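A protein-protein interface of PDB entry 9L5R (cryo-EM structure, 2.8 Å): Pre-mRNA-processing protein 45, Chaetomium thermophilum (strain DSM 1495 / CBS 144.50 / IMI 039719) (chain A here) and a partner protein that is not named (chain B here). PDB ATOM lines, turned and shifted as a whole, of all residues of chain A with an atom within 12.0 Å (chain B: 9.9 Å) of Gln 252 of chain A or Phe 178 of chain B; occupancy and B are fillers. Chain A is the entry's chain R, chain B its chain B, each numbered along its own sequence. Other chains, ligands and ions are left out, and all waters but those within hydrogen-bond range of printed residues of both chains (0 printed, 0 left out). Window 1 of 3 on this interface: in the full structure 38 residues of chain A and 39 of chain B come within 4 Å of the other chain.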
ATOM      1  N   PRO A 244      -2.468  31.464  20.207  1.00  0.00           N
ATOM      2  CA  PRO A 244      -2.429  30.008  20.165  1.00  0.00           C
ATOM      3  C   PRO A 244      -2.156  29.350  18.806  1.00  0.00           C
ATOM      4  O   PRO A 244      -2.587  29.876  17.837  1.00  0.00           O
ATOM      5  CB  PRO A 244      -3.868  29.701  20.557  1.00  0.00           C
ATOM      6  CG  PRO A 244      -4.222  30.781  21.518  1.00  0.00           C
ATOM      7  CD  PRO A 244      -3.682  31.997  20.814  1.00  0.00           C
ATOM      8  N   ARG A 245      -1.489  28.196  18.780  1.00  0.00           N
ATOM      9  CA  ARG A 245      -1.212  27.499  17.538  1.00  0.00           C
ATOM     10  C   ARG A 245      -2.495  26.904  16.983  1.00  0.00           C
ATOM     11  O   ARG A 245      -3.301  26.335  17.718  1.00  0.00           O
ATOM     12  CB  ARG A 245      -0.180  26.410  17.790  1.00  0.00           C
ATOM     13  CG  ARG A 245       0.219  25.595  16.602  1.00  0.00           C
ATOM     14  CD  ARG A 245       1.336  24.668  16.991  1.00  0.00           C
ATOM     15  NE  ARG A 245       1.482  23.523  16.102  1.00  0.00           N
ATOM     16  CZ  ARG A 245       2.420  22.599  16.247  1.00  0.00           C
ATOM     17  NH1 ARG A 245       3.305  22.663  17.228  1.00  0.00           N
ATOM     18  NH2 ARG A 245       2.469  21.582  15.396  1.00  0.00           N
ATOM     19  N   LYS A 246      -2.696  27.050  15.687  1.00  0.00           N
ATOM     20  CA  LYS A 246      -3.887  26.521  15.046  1.00  0.00           C
ATOM     21  C   LYS A 246      -3.625  25.069  14.673  1.00  0.00           C
ATOM     22  O   LYS A 246      -2.822  24.784  13.782  1.00  0.00           O
ATOM     23  CB  LYS A 246      -4.259  27.359  13.830  1.00  0.00           C
ATOM     24  CG  LYS A 246      -4.440  28.820  14.147  1.00  0.00           C
ATOM     25  CD  LYS A 246      -5.142  29.539  13.014  1.00  0.00           C
ATOM     26  CE  LYS A 246      -5.393  31.000  13.345  1.00  0.00           C
ATOM     27  NZ  LYS A 246      -4.152  31.788  13.213  1.00  0.00           N
ATOM     28  N   LEU A 247      -4.293  24.155  15.357  1.00  0.00           N
ATOM     29  CA  LEU A 247      -4.089  22.733  15.156  1.00  0.00           C
ATOM     30  C   LEU A 247      -5.212  22.148  14.328  1.00  0.00           C
ATOM     31  O   LEU A 247      -6.328  22.661  14.295  1.00  0.00           O
ATOM     32  CB  LEU A 247      -4.024  21.992  16.484  1.00  0.00           C
ATOM     33  CG  LEU A 247      -2.969  22.309  17.523  1.00  0.00           C
ATOM     34  CD1 LEU A 247      -3.461  21.728  18.803  1.00  0.00           C
ATOM     35  CD2 LEU A 247      -1.658  21.701  17.122  1.00  0.00           C
ATOM     36  N   THR A 248      -4.908  21.049  13.669  1.00  0.00           N
ATOM     37  CA  THR A 248      -5.906  20.298  12.940  1.00  0.00           C
ATOM     38  C   THR A 248      -6.272  19.035  13.704  1.00  0.00           C
ATOM     39  O   THR A 248      -5.595  18.608  14.652  1.00  0.00           O
ATOM     40  CB  THR A 248      -5.405  19.962  11.532  1.00  0.00           C
ATOM     41  OG1 THR A 248      -4.246  19.126  11.615  1.00  0.00           O
ATOM     42  CG2 THR A 248      -5.041  21.232  10.791  1.00  0.00           C
ATOM     43  N   ALA A 249      -7.377  18.434  13.272  1.00  0.00           N
ATOM     44  CA  ALA A 249      -7.762  17.136  13.800  1.00  0.00           C
ATOM     45  C   ALA A 249      -6.723  16.071  13.472  1.00  0.00           C
ATOM     46  O   ALA A 249      -6.567  15.103  14.220  1.00  0.00           O
ATOM     47  CB  ALA A 249      -9.138  16.751  13.268  1.00  0.00           C
ATOM     48  N   GLU A 250      -5.975  16.255  12.386  1.00  0.00           N
ATOM     49  CA  GLU A 250      -4.872  15.358  12.088  1.00  0.00           C
ATOM     50  C   GLU A 250      -3.722  15.523  13.066  1.00  0.00           C
ATOM     51  O   GLU A 250      -3.051  14.540  13.387  1.00  0.00           O
ATOM     52  CB  GLU A 250      -4.403  15.559  10.651  1.00  0.00           C
ATOM     53  CG  GLU A 250      -5.415  15.129   9.592  1.00  0.00           C
ATOM     54  CD  GLU A 250      -6.481  16.176   9.302  1.00  0.00           C
ATOM     55  OE1 GLU A 250      -6.427  17.284   9.870  1.00  0.00           O
ATOM     56  OE2 GLU A 250      -7.388  15.887   8.504  1.00  0.00           O
ATOM     57  N   ASP A 251      -3.488  16.740  13.566  1.00  0.00           N
ATOM     58  CA  ASP A 251      -2.512  16.933  14.632  1.00  0.00           C
ATOM     59  C   ASP A 251      -2.949  16.239  15.912  1.00  0.00           C
ATOM     60  O   ASP A 251      -2.138  15.579  16.585  1.00  0.00           O
ATOM     61  CB  ASP A 251      -2.295  18.423  14.876  1.00  0.00           C
ATOM     62  CG  ASP A 251      -1.677  19.114  13.698  1.00  0.00           C
ATOM     63  OD1 ASP A 251      -1.113  18.413  12.835  1.00  0.00           O
ATOM     64  OD2 ASP A 251      -1.754  20.349  13.614  1.00  0.00           O
ATOM     65  N   GLN A 252      -4.235  16.356  16.250  1.00  0.00           N
ATOM     66  CA  GLN A 252      -4.746  15.666  17.430  1.00  0.00           C
ATOM     67  C   GLN A 252      -4.607  14.147  17.304  1.00  0.00           C
ATOM     68  O   GLN A 252      -4.152  13.474  18.243  1.00  0.00           O
ATOM     69  CB  GLN A 252      -6.199  16.070  17.673  1.00  0.00           C
ATOM     70  CG  GLN A 252      -6.389  17.548  17.970  1.00  0.00           C
ATOM     71  CD  GLN A 252      -5.976  17.938  19.376  1.00  0.00           C
ATOM     72  OE1 GLN A 252      -5.789  17.086  20.227  1.00  0.00           O
ATOM     73  NE2 GLN A 252      -5.823  19.224  19.616  1.00  0.00           N
ATOM     74  N   GLU A 253      -4.946  13.602  16.137  1.00  0.00           N
ATOM     75  CA  GLU A 253      -4.795  12.170  15.898  1.00  0.00           C
ATOM     76  C   GLU A 253      -3.340  11.737  15.919  1.00  0.00           C
ATOM     77  O   GLU A 253      -3.026  10.636  16.377  1.00  0.00           O
ATOM     78  CB  GLU A 253      -5.423  11.781  14.563  1.00  0.00           C
ATOM     79  CG  GLU A 253      -6.904  11.642  14.639  1.00  0.00           C
ATOM     80  CD  GLU A 253      -7.339  10.683  15.733  1.00  0.00           C
ATOM     81  OE1 GLU A 253      -6.772   9.571  15.822  1.00  0.00           O
ATOM     82  OE2 GLU A 253      -8.242  11.051  16.518  1.00  0.00           O
ATOM     83  N   ALA A 254      -2.440  12.573  15.406  1.00  0.00           N
ATOM     84  CA  ALA A 254      -1.038  12.215  15.386  1.00  0.00           C
ATOM     85  C   ALA A 254      -0.415  12.241  16.763  1.00  0.00           C
ATOM     86  O   ALA A 254       0.661  11.670  16.946  1.00  0.00           O
ATOM     87  CB  ALA A 254      -0.268  13.146  14.466  1.00  0.00           C
ATOM     88  N   TRP A 255      -1.034  12.905  17.729  1.00  0.00           N
ATOM     89  CA  TRP A 255      -0.490  12.869  19.079  1.00  0.00           C
ATOM     90  C   TRP A 255      -1.334  12.095  20.082  1.00  0.00           C
ATOM     91  O   TRP A 255      -1.014  12.116  21.269  1.00  0.00           O
ATOM     92  CB  TRP A 255      -0.251  14.289  19.579  1.00  0.00           C
ATOM     93  CG  TRP A 255       0.890  14.917  18.897  1.00  0.00           C
ATOM     94  CD1 TRP A 255       0.849  15.656  17.773  1.00  0.00           C
ATOM     95  CD2 TRP A 255       2.263  14.831  19.274  1.00  0.00           C
ATOM     96  NE1 TRP A 255       2.104  16.056  17.422  1.00  0.00           N
ATOM     97  CE2 TRP A 255       2.996  15.555  18.328  1.00  0.00           C
ATOM     98  CE3 TRP A 255       2.945  14.214  20.326  1.00  0.00           C
ATOM     99  CZ2 TRP A 255       4.375  15.698  18.405  1.00  0.00           C
ATOM    100  CZ3 TRP A 255       4.311  14.359  20.401  1.00  0.00           C
ATOM    101  CH2 TRP A 255       5.012  15.092  19.445  1.00  0.00           C
ATOM    102  N   ARG A 256      -2.397  11.420  19.656  1.00  0.00           N
ATOM    103  CA  ARG A 256      -3.062  10.482  20.553  1.00  0.00           C
ATOM    104  C   ARG A 256      -2.158   9.285  20.855  1.00  0.00           C
ATOM    105  O   ARG A 256      -1.351   8.864  20.025  1.00  0.00           O
ATOM    106  CB  ARG A 256      -4.387  10.017  19.953  1.00  0.00           C
ATOM    107  CG  ARG A 256      -5.545  10.916  20.355  1.00  0.00           C
ATOM    108  CD  ARG A 256      -6.817  10.647  19.579  1.00  0.00           C
ATOM    109  NE  ARG A 256      -6.930   9.265  19.132  1.00  0.00           N
ATOM    110  CZ  ARG A 256      -7.677   8.352  19.738  1.00  0.00           C
ATOM    111  NH1 ARG A 256      -8.376   8.642  20.823  1.00  0.00           N
ATOM    112  NH2 ARG A 256      -7.736   7.122  19.233  1.00  0.00           N
ATOM    113  N   ILE A 257      -2.297   8.740  22.059  1.00  0.00           N
ATOM    114  CA  ILE A 257      -1.361   7.770  22.618  1.00  0.00           C
ATOM    115  C   ILE A 257      -2.087   6.446  22.810  1.00  0.00           C
ATOM    116  O   ILE A 257      -3.196   6.433  23.341  1.00  0.00           O
ATOM    117  CB  ILE A 257      -0.757   8.256  23.948  1.00  0.00           C
ATOM    118  CG1 ILE A 257       0.052   9.518  23.679  1.00  0.00           C
ATOM    119  CG2 ILE A 257       0.098   7.200  24.595  1.00  0.00           C
ATOM    120  CD1 ILE A 257       0.342  10.341  24.866  1.00  0.00           C
ATOM    121  N   PRO A 258      -1.523   5.330  22.365  1.00  0.00           N
ATOM    122  CA  PRO A 258      -2.166   4.023  22.542  1.00  0.00           C
ATOM    123  C   PRO A 258      -2.298   3.643  24.005  1.00  0.00           C
ATOM    124  O   PRO A 258      -1.419   3.948  24.817  1.00  0.00           O
ATOM    125  CB  PRO A 258      -1.216   3.064  21.822  1.00  0.00           C
ATOM    126  CG  PRO A 258      -0.357   3.888  21.004  1.00  0.00           C
ATOM    127  CD  PRO A 258      -0.316   5.253  21.536  1.00  0.00           C
ATOM    128  N   HIS B 172     -20.174  22.864   8.912  1.00  0.00           N
ATOM    129  CA  HIS B 172     -20.412  22.275  10.227  1.00  0.00           C
ATOM    130  C   HIS B 172     -20.004  20.809  10.260  1.00  0.00           C
ATOM    131  O   HIS B 172     -19.408  20.339  11.242  1.00  0.00           O
ATOM    132  CB  HIS B 172     -21.874  22.408  10.626  1.00  0.00           C
ATOM    133  CG  HIS B 172     -22.314  23.812  10.868  1.00  0.00           C
ATOM    134  ND1 HIS B 172     -23.626  24.208  10.754  1.00  0.00           N
ATOM    135  CD2 HIS B 172     -21.615  24.918  11.202  1.00  0.00           C
ATOM    136  CE1 HIS B 172     -23.720  25.495  11.028  1.00  0.00           C
ATOM    137  NE2 HIS B 172     -22.513  25.951  11.301  1.00  0.00           N
ATOM    138  N   ARG B 173     -20.312  20.075   9.190  1.00  0.00           N
ATOM    139  CA  ARG B 173     -19.933  18.672   9.111  1.00  0.00           C
ATOM    140  C   ARG B 173     -18.422  18.498   9.127  1.00  0.00           C
ATOM    141  O   ARG B 173     -17.905  17.583   9.774  1.00  0.00           O
ATOM    142  CB  ARG B 173     -20.526  18.047   7.860  1.00  0.00           C
ATOM    143  CG  ARG B 173     -21.691  17.142   8.129  1.00  0.00           C
ATOM    144  CD  ARG B 173     -22.010  16.320   6.913  1.00  0.00           C
ATOM    145  NE  ARG B 173     -21.857  17.090   5.688  1.00  0.00           N
ATOM    146  CZ  ARG B 173     -22.830  17.780   5.117  1.00  0.00           C
ATOM    147  NH1 ARG B 173     -24.042  17.826   5.639  1.00  0.00           N
ATOM    148  NH2 ARG B 173     -22.582  18.437   3.990  1.00  0.00           N
ATOM    149  N   ASP B 174     -17.694  19.358   8.418  1.00  0.00           N
ATOM    150  CA  ASP B 174     -16.241  19.273   8.429  1.00  0.00           C
ATOM    151  C   ASP B 174     -15.633  19.744   9.739  1.00  0.00           C
ATOM    152  O   ASP B 174     -14.536  19.306  10.086  1.00  0.00           O
ATOM    153  CB  ASP B 174     -15.644  20.088   7.281  1.00  0.00           C
ATOM    154  CG  ASP B 174     -15.957  19.502   5.921  1.00  0.00           C
ATOM    155  OD1 ASP B 174     -16.386  18.333   5.853  1.00  0.00           O
ATOM    156  OD2 ASP B 174     -15.760  20.210   4.916  1.00  0.00           O
ATOM    157  N   ASP B 175     -16.314  20.615  10.471  1.00  0.00           N
ATOM    158  CA  ASP B 175     -15.788  21.202  11.691  1.00  0.00           C
ATOM    159  C   ASP B 175     -16.299  20.493  12.941  1.00  0.00           C
ATOM    160  O   ASP B 175     -16.111  20.997  14.048  1.00  0.00           O
ATOM    161  CB  ASP B 175     -16.156  22.686  11.713  1.00  0.00           C
ATOM    162  CG  ASP B 175     -15.251  23.514  12.594  1.00  0.00           C
ATOM    163  OD1 ASP B 175     -14.055  23.652  12.269  1.00  0.00           O
ATOM    164  OD2 ASP B 175     -15.755  24.074  13.579  1.00  0.00           O
ATOM    165  N   THR B 176     -16.997  19.369  12.777  1.00  0.00           N
ATOM    166  CA  THR B 176     -17.427  18.574  13.928  1.00  0.00           C
ATOM    167  C   THR B 176     -16.252  18.091  14.776  1.00  0.00           C
ATOM    168  O   THR B 176     -16.267  18.233  16.004  1.00  0.00           O
ATOM    169  CB  THR B 176     -18.254  17.386  13.451  1.00  0.00           C
ATOM    170  OG1 THR B 176     -19.431  17.861  12.798  1.00  0.00           O
ATOM    171  CG2 THR B 176     -18.652  16.510  14.610  1.00  0.00           C
ATOM    172  N   ALA B 177     -15.228  17.517  14.151  1.00  0.00           N
ATOM    173  CA  ALA B 177     -14.135  16.925  14.912  1.00  0.00           C
ATOM    174  C   ALA B 177     -13.301  17.988  15.619  1.00  0.00           C
ATOM    175  O   ALA B 177     -13.163  19.116  15.147  1.00  0.00           O
ATOM    176  CB  ALA B 177     -13.241  16.086  14.009  1.00  0.00           C
ATOM    177  N   PHE B 178     -12.739  17.602  16.762  1.00  0.00           N
ATOM    178  CA  PHE B 178     -12.004  18.527  17.612  1.00  0.00           C
ATOM    179  C   PHE B 178     -10.696  18.947  16.955  1.00  0.00           C
ATOM    180  O   PHE B 178      -9.935  18.111  16.470  1.00  0.00           O
ATOM    181  CB  PHE B 178     -11.735  17.887  18.977  1.00  0.00           C
ATOM    182  CG  PHE B 178     -11.027  18.789  19.948  1.00  0.00           C
ATOM    183  CD1 PHE B 178     -11.734  19.653  20.753  1.00  0.00           C
ATOM    184  CD2 PHE B 178      -9.650  18.758  20.070  1.00  0.00           C
ATOM    185  CE1 PHE B 178     -11.085  20.476  21.643  1.00  0.00           C
ATOM    186  CE2 PHE B 178      -9.008  19.585  20.950  1.00  0.00           C
ATOM    187  CZ  PHE B 178      -9.726  20.443  21.734  1.00  0.00           C
ATOM    188  N   ARG B 179     -10.433  20.246  16.954  1.00  0.00           N
ATOM    189  CA  ARG B 179      -9.150  20.770  16.512  1.00  0.00           C
ATOM    190  C   ARG B 179      -8.399  21.460  17.635  1.00  0.00           C
ATOM    191  O   ARG B 179      -7.253  21.106  17.908  1.00  0.00           O
ATOM    192  CB  ARG B 179      -9.352  21.717  15.324  1.00  0.00           C
ATOM    193  CG  ARG B 179      -9.602  20.937  14.077  1.00  0.00           C
ATOM    194  CD  ARG B 179     -10.540  21.592  13.119  1.00  0.00           C
ATOM    195  NE  ARG B 179     -10.258  23.005  12.950  1.00  0.00           N
ATOM    196  CZ  ARG B 179     -10.758  23.737  11.968  1.00  0.00           C
ATOM    197  NH1 ARG B 179     -11.608  23.226  11.094  1.00  0.00           N
ATOM    198  NH2 ARG B 179     -10.391  25.011  11.858  1.00  0.00           N
ATOM    199  N   ASP B 180      -9.015  22.440  18.286  1.00  0.00           N
ATOM    200  CA  ASP B 180      -8.461  23.062  19.477  1.00  0.00           C
ATOM    201  C   ASP B 180      -9.566  23.816  20.190  1.00  0.00           C
ATOM    202  O   ASP B 180     -10.699  23.936  19.706  1.00  0.00           O
ATOM    203  CB  ASP B 180      -7.275  23.991  19.170  1.00  0.00           C
ATOM    204  CG  ASP B 180      -7.525  24.903  18.012  1.00  0.00           C
ATOM    205  OD1 ASP B 180      -8.603  24.839  17.425  1.00  0.00           O
ATOM    206  OD2 ASP B 180      -6.633  25.693  17.672  1.00  0.00           O
ATOM    207  N   TYR B 181      -9.211  24.336  21.357  1.00  0.00           N
ATOM    208  CA  TYR B 181     -10.201  24.986  22.188  1.00  0.00           C
ATOM    209  C   TYR B 181     -10.596  26.348  21.655  1.00  0.00           C
ATOM    210  O   TYR B 181     -11.690  26.807  21.968  1.00  0.00           O
ATOM    211  CB  TYR B 181      -9.701  25.067  23.620  1.00  0.00           C
ATOM    212  CG  TYR B 181      -9.918  23.772  24.354  1.00  0.00           C
ATOM    213  CD1 TYR B 181     -11.197  23.304  24.597  1.00  0.00           C
ATOM    214  CD2 TYR B 181      -8.851  23.008  24.783  1.00  0.00           C
ATOM    215  CE1 TYR B 181     -11.407  22.128  25.250  1.00  0.00           C
ATOM    216  CE2 TYR B 181      -9.049  21.826  25.435  1.00  0.00           C
ATOM    217  CZ  TYR B 181     -10.332  21.391  25.674  1.00  0.00           C
ATOM    218  OH  TYR B 181     -10.556  20.214  26.329  1.00  0.00           O
ATOM    219  N   ALA B 182      -9.766  26.977  20.826  1.00  0.00           N
ATOM    220  CA  ALA B 182     -10.184  28.206  20.165  1.00  0.00           C
ATOM    221  C   ALA B 182     -11.328  27.957  19.191  1.00  0.00           C
ATOM    222  O   ALA B 182     -12.287  28.736  19.144  1.00  0.00           O
ATOM    223  CB  ALA B 182      -8.996  28.846  19.460  1.00  0.00           C
ATOM    224  N   ARG B 183     -11.268  26.861  18.424  1.00  0.00           N
ATOM    225  CA  ARG B 183     -12.397  26.504  17.569  1.00  0.00           C
ATOM    226  C   ARG B 183     -13.613  26.099  18.371  1.00  0.00           C
ATOM    227  O   ARG B 183     -14.733  26.438  17.991  1.00  0.00           O
ATOM    228  CB  ARG B 183     -12.048  25.390  16.584  1.00  0.00           C
ATOM    229  CG  ARG B 183     -11.035  25.834  15.662  1.00  0.00           C
ATOM    230  CD  ARG B 183     -11.627  26.876  14.769  1.00  0.00           C
ATOM    231  NE  ARG B 183     -10.662  27.292  13.769  1.00  0.00           N
ATOM    232  CZ  ARG B 183      -9.827  28.301  13.972  1.00  0.00           C
ATOM    233  NH1 ARG B 183      -9.762  28.914  15.147  1.00  0.00           N
ATOM    234  NH2 ARG B 183      -9.012  28.678  12.991  1.00  0.00           N
ATOM    235  N   GLU B 184     -13.424  25.358  19.461  1.00  0.00           N
ATOM    236  CA  GLU B 184     -14.586  24.978  20.256  1.00  0.00           C
ATOM    237  C   GLU B 184     -15.251  26.197  20.878  1.00  0.00           C
ATOM    238  O   GLU B 184     -16.481  26.273  20.945  1.00  0.00           O
ATOM    239  CB  GLU B 184     -14.198  23.969  21.326  1.00  0.00           C
ATOM    240  CG  GLU B 184     -13.693  22.679  20.776  1.00  0.00           C
ATOM    241  CD  GLU B 184     -14.783  21.809  20.194  1.00  0.00           C
ATOM    242  OE1 GLU B 184     -15.867  21.712  20.804  1.00  0.00           O
ATOM    243  OE2 GLU B 184     -14.550  21.204  19.128  1.00  0.00           O
ATOM    244  N   ALA B 185     -14.454  27.173  21.311  1.00  0.00           N
ATOM    245  CA  ALA B 185     -14.998  28.396  21.884  1.00  0.00           C
ATOM    246  C   ALA B 185     -15.730  29.229  20.844  1.00  0.00           C
ATOM    247  O   ALA B 185     -16.796  29.779  21.132  1.00  0.00           O
ATOM    248  CB  ALA B 185     -13.881  29.204  22.532  1.00  0.00           C
ATOM    249  N   LYS B 187     -17.193  28.036  18.078  1.00  0.00           N
ATOM    250  CA  LYS B 187     -18.418  27.310  17.756  1.00  0.00           C
ATOM    251  C   LYS B 187     -19.470  27.484  18.834  1.00  0.00           C
ATOM    252  O   LYS B 187     -20.655  27.671  18.533  1.00  0.00           O
ATOM    253  CB  LYS B 187     -18.135  25.824  17.591  1.00  0.00           C
ATOM    254  CG  LYS B 187     -17.401  25.417  16.368  1.00  0.00           C
ATOM    255  CD  LYS B 187     -16.674  24.122  16.643  1.00  0.00           C
ATOM    256  CE  LYS B 187     -17.635  22.990  16.879  1.00  0.00           C
ATOM    257  NZ  LYS B 187     -16.929  21.679  16.901  1.00  0.00           N
ATOM    258  N   THR B 188     -19.053  27.414  20.098  1.00  0.00           N
ATOM    259  CA  THR B 188     -19.987  27.551  21.202  1.00  0.00           C
ATOM    260  C   THR B 188     -20.574  28.947  21.251  1.00  0.00           C
ATOM    261  O   THR B 188     -21.776  29.105  21.478  1.00  0.00           O
ATOM    262  CB  THR B 188     -19.282  27.204  22.510  1.00  0.00           C
ATOM    263  OG1 THR B 188     -18.732  25.890  22.407  1.00  0.00           O
ATOM    264  CG2 THR B 188     -20.228  27.248  23.673  1.00  0.00           C
ATOM    265  N   PHE B 308      -8.846   1.868  19.714  1.00  0.00           N
ATOM    266  CA  PHE B 308      -7.508   2.171  19.236  1.00  0.00           C
ATOM    267  C   PHE B 308      -6.880   1.078  18.385  1.00  0.00           C
ATOM    268  O   PHE B 308      -6.302   1.381  17.341  1.00  0.00           O
ATOM    269  CB  PHE B 308      -6.578   2.463  20.406  1.00  0.00           C
ATOM    270  CG  PHE B 308      -5.518   3.432  20.071  1.00  0.00           C
ATOM    271  CD1 PHE B 308      -4.350   3.016  19.459  1.00  0.00           C
ATOM    272  CD2 PHE B 308      -5.699   4.770  20.322  1.00  0.00           C
ATOM    273  CE1 PHE B 308      -3.387   3.919  19.120  1.00  0.00           C
ATOM    274  CE2 PHE B 308      -4.738   5.672  19.997  1.00  0.00           C
ATOM    275  CZ  PHE B 308      -3.579   5.249  19.394  1.00  0.00           C
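Among the printed residues, merely in contact across the chains: Lys 246 of chain A with Asp 180 of chain B, Lys 246 of chain A with Arg 183 of chain B, Leu 247 of chain A with Arg 179 of chain B, Leu 247 of chain A with Asp 180 of chain B, Thr 248 of chain A with Arg 179 of chain B, Ala 249 of chain A with Phe 178 of chain B, Ala 249 of chain A with Arg 179 of chain B, Gln 252 of chain A with Phe 178 of chain B, Arg 256 of chain A with Phe 308 of chain B, Ile 257 of chain A with Phe 308 of chain B and Pro 258 of chain A with Phe 308 of chain B.
O of Arg 179 of chain B sits at hydrogen-bond distance from NE2 of Gln 252 of chain A.
O of Arg 245 of chain A lies close to OD2 of Asp 180 of chain B, 3.4 Å away.
Printed residues of chain B that touch a printed residue of chain A: Phe 178, Arg 179, Asp 180, Arg 183 and Phe 308.
Of the 15 printed residues of chain A, 9 touch a printed residue of chain B.
Hydrophobic or aromatic side chains of chain A within 4 Å of the printed part of chain B: Leu 247, Ala 249 and Pro 258.
Among the printed residues, no Asp or Glu carboxylate lies within 4 Å of a Lys or Arg side-chain nitrogen of the other chain.
The side-chain hydroxyl of Thr 248 of chain A sits close to the side-chain carboxylate of Glu 250 of chain A (3.3 Å).
N of Asp 251 of chain A sits at hydrogen-bond distance from OG1 of Thr 248 of chain A.
The guanidinium group (NE) of Arg 256 of chain A lies within salt-bridge range of the side-chain carboxylate (OE1) of Glu 253 of chain A (3.3 Å).
The side-chain carboxylate (OD1) of Asp 175 of chain B lies within salt-bridge range of the guanidinium group (NH1) of Arg 179 of chain B (2.7 Å).
The backbone NH of Arg 183 of chain B sits close to the side-chain carboxylate of Asp 180 of chain B.
Of the printed residues of chain B, Thr 248 of chain A touches Arg 179 (3.9 Å).
Of chain B, only Phe 178 (3.6 Å) and Arg 179 (3.4 Å) come within 4 Å of Ala 249 of chain A.
No residue of chain B comes within 4 Å of Asp 251 of chain A.
Gln 252 of chain A touches just these residues of chain B: Phe 178 and Arg 179.
No residue of chain B comes within 4 Å of Glu 253 of chain A.
Printed residues of chain B within 4 Å of Ile 257 of chain A: Phe 308.
His 172 of chain B touches none of the printed residues of chain A.
Arg 179 of chain B touches just these residues of chain A: Leu 247 (3.3 Å), Thr 248 (3.9 Å), Ala 249 (3.4 Å) and Gln 252 (2.9 Å).
Asp 180 of chain B touches just these residues of chain A: Arg 245, Lys 246 and Leu 247.
No residue of chain A comes within 4 Å of Tyr 181 of chain B.
Of the printed residues of chain A, Arg 183 of chain B touches Lys 246 (3.96 Å).
Lys 187 of chain B touches none of the printed residues of chain A.
The nearest residue of chain A that does not touch Phe 178 of chain B is Thr 248 of chain A (4.7 Å).
The nearest printed residue of chain B that does not touch Lys 246 of chain A is Arg 179 of chain B (6.3 Å).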
